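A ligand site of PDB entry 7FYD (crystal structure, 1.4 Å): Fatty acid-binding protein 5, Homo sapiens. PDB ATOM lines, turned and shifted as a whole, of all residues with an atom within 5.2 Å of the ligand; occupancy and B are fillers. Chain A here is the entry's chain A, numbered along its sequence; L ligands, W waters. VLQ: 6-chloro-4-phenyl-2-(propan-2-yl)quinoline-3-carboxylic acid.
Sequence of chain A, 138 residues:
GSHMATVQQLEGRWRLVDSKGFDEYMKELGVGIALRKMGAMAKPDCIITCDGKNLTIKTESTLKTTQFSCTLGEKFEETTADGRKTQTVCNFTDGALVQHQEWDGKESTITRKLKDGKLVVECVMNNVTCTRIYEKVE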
ATOM      1  N   PHE A  22      29.425  15.689   8.273  1.00  0.00           N
ATOM      2  CA  PHE A  22      29.170  16.615   7.170  1.00  0.00           C
ATOM      3  C   PHE A  22      29.883  16.205   5.898  1.00  0.00           C
ATOM      4  O   PHE A  22      29.295  16.234   4.832  1.00  0.00           O
ATOM      5  CB  PHE A  22      29.448  18.071   7.594  1.00  0.00           C
ATOM      6  CG  PHE A  22      29.060  19.102   6.514  1.00  0.00           C
ATOM      7  CD1 PHE A  22      27.741  19.247   6.113  1.00  0.00           C
ATOM      8  CD2 PHE A  22      30.014  19.902   5.932  1.00  0.00           C
ATOM      9  CE1 PHE A  22      27.385  20.180   5.163  1.00  0.00           C
ATOM     10  CE2 PHE A  22      29.651  20.899   5.035  1.00  0.00           C
ATOM     11  CZ  PHE A  22      28.370  20.952   4.580  1.00  0.00           C
ATOM     12  N   TYR A  25      28.000  13.364   4.349  1.00  0.00           N
ATOM     13  CA  TYR A  25      26.769  13.892   3.735  1.00  0.00           C
ATOM     14  C   TYR A  25      27.089  14.499   2.349  1.00  0.00           C
ATOM     15  O   TYR A  25      26.416  14.242   1.331  1.00  0.00           O
ATOM     16  CB  TYR A  25      26.091  14.883   4.729  1.00  0.00           C
ATOM     17  CG  TYR A  25      24.883  15.527   4.183  1.00  0.00           C
ATOM     18  CD1 TYR A  25      23.720  14.812   3.974  1.00  0.00           C
ATOM     19  CD2 TYR A  25      24.887  16.857   3.850  1.00  0.00           C
ATOM     20  CE1 TYR A  25      22.568  15.436   3.416  1.00  0.00           C
ATOM     21  CE2 TYR A  25      23.782  17.479   3.310  1.00  0.00           C
ATOM     22  CZ  TYR A  25      22.612  16.787   3.122  1.00  0.00           C
ATOM     23  OH  TYR A  25      21.519  17.452   2.585  1.00  0.00           O
ATOM     24  N   MET A  26      28.167  15.322   2.316  1.00  0.00           N
ATOM     25  CA  MET A  26      28.523  15.952   1.063  1.00  0.00           C
ATOM     26  C   MET A  26      28.942  14.910   0.011  1.00  0.00           C
ATOM     27  O   MET A  26      28.604  15.051  -1.137  1.00  0.00           O
ATOM     28  CB  MET A  26      29.647  16.973   1.242  1.00  0.00           C
ATOM     29  CG  MET A  26      29.279  18.258   1.938  1.00  0.00           C
ATOM     30  SD  MET A  26      30.603  19.551   1.763  1.00  0.00           S
ATOM     31  CE  MET A  26      31.827  18.792   2.817  1.00  0.00           C
ATOM     32  N   LEU A  29      25.743  13.484  -1.375  1.00  0.00           N
ATOM     33  CA  LEU A  29      25.178  14.440  -2.338  1.00  0.00           C
ATOM     34  C   LEU A  29      25.937  14.350  -3.693  1.00  0.00           C
ATOM     35  O   LEU A  29      25.338  14.491  -4.744  1.00  0.00           O
ATOM     36  CB  LEU A  29      25.279  15.862  -1.789  1.00  0.00           C
ATOM     37  CG  LEU A  29      24.335  16.290  -0.697  1.00  0.00           C
ATOM     38  CD1 LEU A  29      24.717  17.688  -0.213  1.00  0.00           C
ATOM     39  CD2 LEU A  29      22.835  16.247  -1.122  1.00  0.00           C
ATOM     40  N   VAL A  31      29.045  16.009  -4.034  1.00  0.00           N
ATOM     41  CA  VAL A  31      29.817  17.233  -4.062  1.00  0.00           C
ATOM     42  C   VAL A  31      31.267  16.905  -4.448  1.00  0.00           C
ATOM     43  O   VAL A  31      31.879  16.018  -3.824  1.00  0.00           O
ATOM     44  CB  VAL A  31      29.757  17.956  -2.667  1.00  0.00           C
ATOM     45  CG1 VAL A  31      30.584  19.246  -2.604  1.00  0.00           C
ATOM     46  CG2 VAL A  31      28.325  18.315  -2.270  1.00  0.00           C
ATOM     47  N   LEU A  35      34.512  21.959  -3.513  1.00  0.00           N
ATOM     48  CA  LEU A  35      33.518  22.335  -2.491  1.00  0.00           C
ATOM     49  C   LEU A  35      33.554  21.525  -1.193  1.00  0.00           C
ATOM     50  O   LEU A  35      33.221  22.026  -0.091  1.00  0.00           O
ATOM     51  CB  LEU A  35      32.096  22.241  -3.100  1.00  0.00           C
ATOM     52  CG  LEU A  35      31.569  23.517  -3.757  1.00  0.00           C
ATOM     53  CD1 LEU A  35      30.115  23.369  -4.205  1.00  0.00           C
ATOM     54  CD2 LEU A  35      31.715  24.802  -2.867  1.00  0.00           C
ATOM     55  N   GLY A  39      33.781  23.164   2.450  1.00  0.00           N
ATOM     56  CA  GLY A  39      32.832  22.795   3.547  1.00  0.00           C
ATOM     57  C   GLY A  39      33.473  22.120   4.764  1.00  0.00           C
ATOM     58  O   GLY A  39      33.004  22.247   5.898  1.00  0.00           O
ATOM     59  N   ALA A  42      35.213  25.577   6.254  1.00  0.00           N
ATOM     60  CA  ALA A  42      34.402  26.724   6.690  1.00  0.00           C
ATOM     61  C   ALA A  42      33.815  26.516   8.120  1.00  0.00           C
ATOM     62  O   ALA A  42      33.484  25.388   8.575  1.00  0.00           O
ATOM     63  CB  ALA A  42      33.295  27.008   5.695  1.00  0.00           C
ATOM     64  N   PRO A  44      30.855  28.487   9.288  1.00  0.00           N
ATOM     65  CA  PRO A  44      29.928  29.537   8.950  1.00  0.00           C
ATOM     66  C   PRO A  44      29.132  30.017  10.140  1.00  0.00           C
ATOM     67  O   PRO A  44      28.999  29.298  11.189  1.00  0.00           O
ATOM     68  CB  PRO A  44      28.991  28.818   7.951  1.00  0.00           C
ATOM     69  CG  PRO A  44      29.085  27.417   8.299  1.00  0.00           C
ATOM     70  CD  PRO A  44      30.443  27.185   8.756  1.00  0.00           C
ATOM     71  N   THR A  59      23.520  31.473   5.167  1.00  0.00           N
ATOM     72  CA  THR A  59      24.700  30.839   5.707  1.00  0.00           C
ATOM     73  C   THR A  59      25.928  31.560   5.184  1.00  0.00           C
ATOM     74  O   THR A  59      26.097  31.715   3.999  1.00  0.00           O
ATOM     75  CB  THR A  59      24.764  29.388   5.198  1.00  0.00           C
ATOM     76  OG1 THR A  59      23.610  28.727   5.732  1.00  0.00           O
ATOM     77  CG2 THR A  59      26.112  28.770   5.552  1.00  0.00           C
ATOM     78  N   SER A  61      30.113  32.608   5.400  1.00  0.00           N
ATOM     79  CA  SER A  61      31.518  32.426   5.710  1.00  0.00           C
ATOM     80  C   SER A  61      32.345  33.083   4.602  1.00  0.00           C
ATOM     81  O   SER A  61      31.826  33.337   3.521  1.00  0.00           O
ATOM     82  CB  SER A  61      31.843  30.930   5.891  1.00  0.00           C
ATOM     83  OG  SER A  61      31.810  30.187   4.710  1.00  0.00           O
ATOM     84  N   LYS A  64      32.367  30.469   1.653  1.00  0.00           N
ATOM     85  CA  LYS A  64      31.101  30.259   0.930  1.00  0.00           C
ATOM     86  C   LYS A  64      29.927  30.936   1.673  1.00  0.00           C
ATOM     87  O   LYS A  64      29.758  30.758   2.883  1.00  0.00           O
ATOM     88  CB  LYS A  64      30.851  28.765   0.820  1.00  0.00           C
ATOM     89  CG  LYS A  64      29.465  28.389   0.310  1.00  0.00           C
ATOM     90  CD  LYS A  64      29.257  28.712  -1.158  1.00  0.00           C
ATOM     91  CE  LYS A  64      29.034  27.454  -1.983  1.00  0.00           C
ATOM     92  NZ  LYS A  64      28.659  27.841  -3.343  1.00  0.00           N
ATOM     93  N   THR A  65      29.100  31.675   0.924  1.00  0.00           N
ATOM     94  CA  THR A  65      27.822  32.247   1.478  1.00  0.00           C
ATOM     95  C   THR A  65      26.674  31.862   0.537  1.00  0.00           C
ATOM     96  O   THR A  65      26.823  31.911  -0.662  1.00  0.00           O
ATOM     97  CB  THR A  65      27.934  33.769   1.559  1.00  0.00           C
ATOM     98  OG1 THR A  65      28.886  34.124   2.560  1.00  0.00           O
ATOM     99  CG2 THR A  65      26.612  34.462   1.906  1.00  0.00           C
ATOM    100  N   THR A  66      25.548  31.473   1.113  1.00  0.00           N
ATOM    101  CA  THR A  66      24.304  31.150   0.377  1.00  0.00           C
ATOM    102  C   THR A  66      23.119  31.716   1.192  1.00  0.00           C
ATOM    103  O   THR A  66      23.231  31.945   2.385  1.00  0.00           O
ATOM    104  CB  THR A  66      24.096  29.644   0.183  1.00  0.00           C
ATOM    105  OG1 THR A  66      23.928  29.001   1.446  1.00  0.00           O
ATOM    106  CG2 THR A  66      25.286  29.006  -0.570  1.00  0.00           C
ATOM    107  N   ALA A  81      23.893  25.243  -1.966  1.00  0.00           N
ATOM    108  CA  ALA A  81      25.337  25.592  -1.946  1.00  0.00           C
ATOM    109  C   ALA A  81      26.130  24.903  -3.039  1.00  0.00           C
ATOM    110  O   ALA A  81      27.083  25.430  -3.651  1.00  0.00           O
ATOM    111  CB  ALA A  81      25.929  25.280  -0.615  1.00  0.00           C
ATOM    112  N   ASP A  82      25.778  23.663  -3.301  1.00  0.00           N
ATOM    113  CA  ASP A  82      26.495  22.850  -4.238  1.00  0.00           C
ATOM    114  C   ASP A  82      25.822  22.866  -5.619  1.00  0.00           C
ATOM    115  O   ASP A  82      26.190  22.097  -6.532  1.00  0.00           O
ATOM    116  CB  ASP A  82      26.605  21.414  -3.686  1.00  0.00           C
ATOM    117  CG  ASP A  82      25.243  20.778  -3.389  1.00  0.00           C
ATOM    118  OD1 ASP A  82      24.456  21.418  -2.627  1.00  0.00           O
ATOM    119  OD2 ASP A  82      24.977  19.679  -3.891  1.00  0.00           O
ATOM    120  N   ARG A  84      22.600  22.353  -6.808  1.00  0.00           N
ATOM    121  CA  ARG A  84      21.366  21.662  -7.164  1.00  0.00           C
ATOM    122  C   ARG A  84      20.213  22.672  -7.280  1.00  0.00           C
ATOM    123  O   ARG A  84      20.180  23.663  -6.572  1.00  0.00           O
ATOM    124  CB  ARG A  84      20.980  20.601  -6.138  1.00  0.00           C
ATOM    125  CG  ARG A  84      21.899  19.416  -5.990  1.00  0.00           C
ATOM    126  CD  ARG A  84      21.628  18.557  -4.817  1.00  0.00           C
ATOM    127  NE  ARG A  84      22.145  19.170  -3.602  1.00  0.00           N
ATOM    128  CZ  ARG A  84      21.558  19.334  -2.437  1.00  0.00           C
ATOM    129  NH1 ARG A  84      20.325  18.848  -2.239  1.00  0.00           N
ATOM    130  NH2 ARG A  84      22.199  19.982  -1.486  1.00  0.00           N
ATOM    131  N   ILE A 110      16.543  18.317   6.071  1.00  0.00           N
ATOM    132  CA  ILE A 110      17.353  19.121   6.990  1.00  0.00           C
ATOM    133  C   ILE A 110      16.436  19.642   8.080  1.00  0.00           C
ATOM    134  O   ILE A 110      15.439  20.306   7.795  1.00  0.00           O
ATOM    135  CB  ILE A 110      17.983  20.362   6.271  1.00  0.00           C
ATOM    136  CG1 ILE A 110      18.957  19.927   5.128  1.00  0.00           C
ATOM    137  CG2 ILE A 110      18.733  21.286   7.250  1.00  0.00           C
ATOM    138  CD1 ILE A 110      18.870  20.825   3.889  1.00  0.00           C
ATOM    139  N   ARG A 112      16.110  21.820  11.888  1.00  0.00           N
ATOM    140  CA  ARG A 112      16.768  22.841  12.700  1.00  0.00           C
ATOM    141  C   ARG A 112      15.904  23.066  13.924  1.00  0.00           C
ATOM    142  O   ARG A 112      14.695  23.276  13.803  1.00  0.00           O
ATOM    143  CB  ARG A 112      16.936  24.144  11.933  1.00  0.00           C
ATOM    144  CG  ARG A 112      17.753  24.038  10.677  1.00  0.00           C
ATOM    145  CD  ARG A 112      18.006  25.406  10.035  1.00  0.00           C
ATOM    146  NE  ARG A 112      18.787  25.343   8.822  1.00  0.00           N
ATOM    147  CZ  ARG A 112      18.396  24.997   7.588  1.00  0.00           C
ATOM    148  NH1 ARG A 112      17.204  24.592   7.296  1.00  0.00           N
ATOM    149  NH2 ARG A 112      19.313  25.060   6.623  1.00  0.00           N
ATOM    150  N   VAL A 121      21.364  21.558  13.950  1.00  0.00           N
ATOM    151  CA  VAL A 121      21.044  21.301  12.540  1.00  0.00           C
ATOM    152  C   VAL A 121      21.400  19.846  12.195  1.00  0.00           C
ATOM    153  O   VAL A 121      22.512  19.408  12.401  1.00  0.00           O
ATOM    154  CB  VAL A 121      21.747  22.244  11.595  1.00  0.00           C
ATOM    155  CG1 VAL A 121      21.385  21.925  10.089  1.00  0.00           C
ATOM    156  CG2 VAL A 121      21.488  23.752  11.947  1.00  0.00           C
ATOM    157  N   CYS A 123      21.011  16.754   9.115  1.00  0.00           N
ATOM    158  CA  CYS A 123      20.775  16.484   7.708  1.00  0.00           C
ATOM    159  C   CYS A 123      20.833  15.013   7.437  1.00  0.00           C
ATOM    160  O   CYS A 123      21.519  14.280   8.108  1.00  0.00           O
ATOM    161  CB  CYS A 123      21.788  17.134   6.814  1.00  0.00           C
ATOM    162  SG  CYS A 123      21.995  18.875   7.148  1.00  0.00           S
ATOM    163  N   ARG A 132      25.198  19.315  13.071  1.00  0.00           N
ATOM    164  CA  ARG A 132      25.983  20.531  13.235  1.00  0.00           C
ATOM    165  C   ARG A 132      25.330  21.375  14.343  1.00  0.00           C
ATOM    166  O   ARG A 132      24.089  21.575  14.334  1.00  0.00           O
ATOM    167  CB  ARG A 132      26.014  21.310  11.925  1.00  0.00           C
ATOM    168  CG  ARG A 132      26.900  20.582  10.920  1.00  0.00           C
ATOM    169  CD  ARG A 132      26.769  20.874   9.445  1.00  0.00           C
ATOM    170  NE  ARG A 132      27.262  22.142   8.946  1.00  0.00           N
ATOM    171  CZ  ARG A 132      28.557  22.446   8.705  1.00  0.00           C
ATOM    172  NH1 ARG A 132      29.564  21.684   9.064  1.00  0.00           N
ATOM    173  NH2 ARG A 132      28.817  23.617   8.160  1.00  0.00           N
ATOM    174  N   TYR A 134      25.333  25.018  16.675  1.00  0.00           N
ATOM    175  CA  TYR A 134      25.636  26.453  16.611  1.00  0.00           C
ATOM    176  C   TYR A 134      25.298  27.149  17.915  1.00  0.00           C
ATOM    177  O   TYR A 134      24.311  26.826  18.556  1.00  0.00           O
ATOM    178  CB  TYR A 134      24.877  27.153  15.453  1.00  0.00           C
ATOM    179  CG  TYR A 134      25.135  26.607  14.037  1.00  0.00           C
ATOM    180  CD1 TYR A 134      24.596  25.379  13.622  1.00  0.00           C
ATOM    181  CD2 TYR A 134      25.816  27.358  13.071  1.00  0.00           C
ATOM    182  CE1 TYR A 134      24.829  24.903  12.337  1.00  0.00           C
ATOM    183  CE2 TYR A 134      26.004  26.884  11.793  1.00  0.00           C
ATOM    184  CZ  TYR A 134      25.500  25.651  11.425  1.00  0.00           C
ATOM    185  OH  TYR A 134      25.674  25.067  10.169  1.00  0.00           O
HETATM  186  C1  VLQ L   1      27.566  22.186   0.570  1.00  0.00           C
HETATM  187  C2  VLQ L   1      26.609  21.189   0.434  1.00  0.00           C
HETATM  188  C3  VLQ L   1      25.612  21.102   1.354  1.00  0.00           C
HETATM  189  C4  VLQ L   1      27.547  23.135   1.547  1.00  0.00           C
HETATM  190  C5  VLQ L   1      27.472  25.025   3.708  1.00  0.00           C
HETATM  191  C6  VLQ L   1      27.396  26.320   3.160  1.00  0.00           C
HETATM  192  C7  VLQ L   1      28.449  27.216   3.426  1.00  0.00           C
HETATM  193  C8  VLQ L   1      29.545  26.858   4.189  1.00  0.00           C
HETATM  194  C9  VLQ L   1      29.579  25.600   4.739  1.00  0.00           C
HETATM  195  C10 VLQ L   1      28.548  24.704   4.529  1.00  0.00           C
HETATM  196 CL11 VLQ L   1      28.775  22.299  -0.621  1.00  0.00          CL
HETATM  197  C12 VLQ L   1      26.525  23.073   2.505  1.00  0.00           C
HETATM  198  C13 VLQ L   1      25.537  22.050   2.392  1.00  0.00           C
HETATM  199  N14 VLQ L   1      24.538  21.879   3.305  1.00  0.00           N
HETATM  200  C15 VLQ L   1      24.469  22.741   4.291  1.00  0.00           C
HETATM  201  C16 VLQ L   1      25.420  23.834   4.483  1.00  0.00           C
HETATM  202  C17 VLQ L   1      26.434  24.013   3.556  1.00  0.00           C
HETATM  203  C18 VLQ L   1      23.343  22.572   5.285  1.00  0.00           C
HETATM  204  C19 VLQ L   1      21.959  22.575   4.644  1.00  0.00           C
HETATM  205  C20 VLQ L   1      23.717  21.341   6.069  1.00  0.00           C
HETATM  206  C21 VLQ L   1      25.240  24.798   5.629  1.00  0.00           C
HETATM  207  O22 VLQ L   1      24.282  25.706   5.327  1.00  0.00           O
HETATM  208  O23 VLQ L   1      25.807  24.882   6.708  1.00  0.00           O
HETATM  209  O   HOH W   1      23.850  24.288   8.735  1.00  0.00           O
HETATM  210  O   HOH W   2      23.451  26.051   2.799  1.00  0.00           O
HETATM  211  O   HOH W   3      22.199  26.531   6.419  1.00  0.00           O
HETATM  212  O   HOH W   4      25.819  27.118   8.317  1.00  0.00           O
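Residues that only touch the ligand: Phe 22, Leu 29, Leu 35, Lys 64, Ala 81, Asp 82, Ile 110 and Cys 123.
Hydrophobic or aromatic side chains that line the ligand: Phe 22, Leu 29, Leu 35, Ala 81 and Ile 110.
11 residues have an atom within 4 Å of the ligand: Phe 22, Leu 29, Leu 35, Thr 59, Lys 64, Ala 81, Asp 82, Ile 110, Cys 123, Arg 132 and Tyr 134.
Along chain A the residues within 4 Å of the ligand span positions 22 to 134.
The nearest printed residue that does not touch the ligand is Pro 44 (4.03 Å).
Water W3 lies within hydrogen-bond range of an oxygen (O22) of the ligand, the side-chain hydroxyl (OG1) of Thr 59 and the guanidinium group (NH2) of Arg 112.
Water W2 bridges O22 of the ligand and OG1 of Thr 66.
Water W4 bridges an oxygen (O23) of the ligand and the side-chain hydroxyl (OH) of Tyr 134.
Water W1 lies within hydrogen-bond range of the side-chain hydroxyl (OH) of Tyr 134 and an oxygen (O23) of the ligand.
An oxygen (O22) of the ligand sits at hydrogen-bond distance from the side-chain hydroxyl (OG1) of Thr 59 (3.1 Å).
O23 of the ligand lies within hydrogen-bond range of OH of Tyr 134 (3.5 Å).
NH2 of Arg 132 lies within salt-bridge range of O23 of the ligand (3.6 Å).
N of Thr 59 is in hydrogen-bond range of O of Thr 66 (2.8 Å).
The backbone carbonyl oxygen (O) of Ala 81 sits at hydrogen-bond distance from the side-chain amino group (NZ) of Lys 64.
The side-chain hydroxyl of Ser 61 sits at hydrogen-bond distance from the backbone carbonyl oxygen of Lys 64 (2.8 Å).
The backbone NH of Val 121 sits at hydrogen-bond distance from the backbone carbonyl oxygen of Arg 132 (2.8 Å).
NE of Arg 84 lies within salt-bridge range of OD2 of Asp 82.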
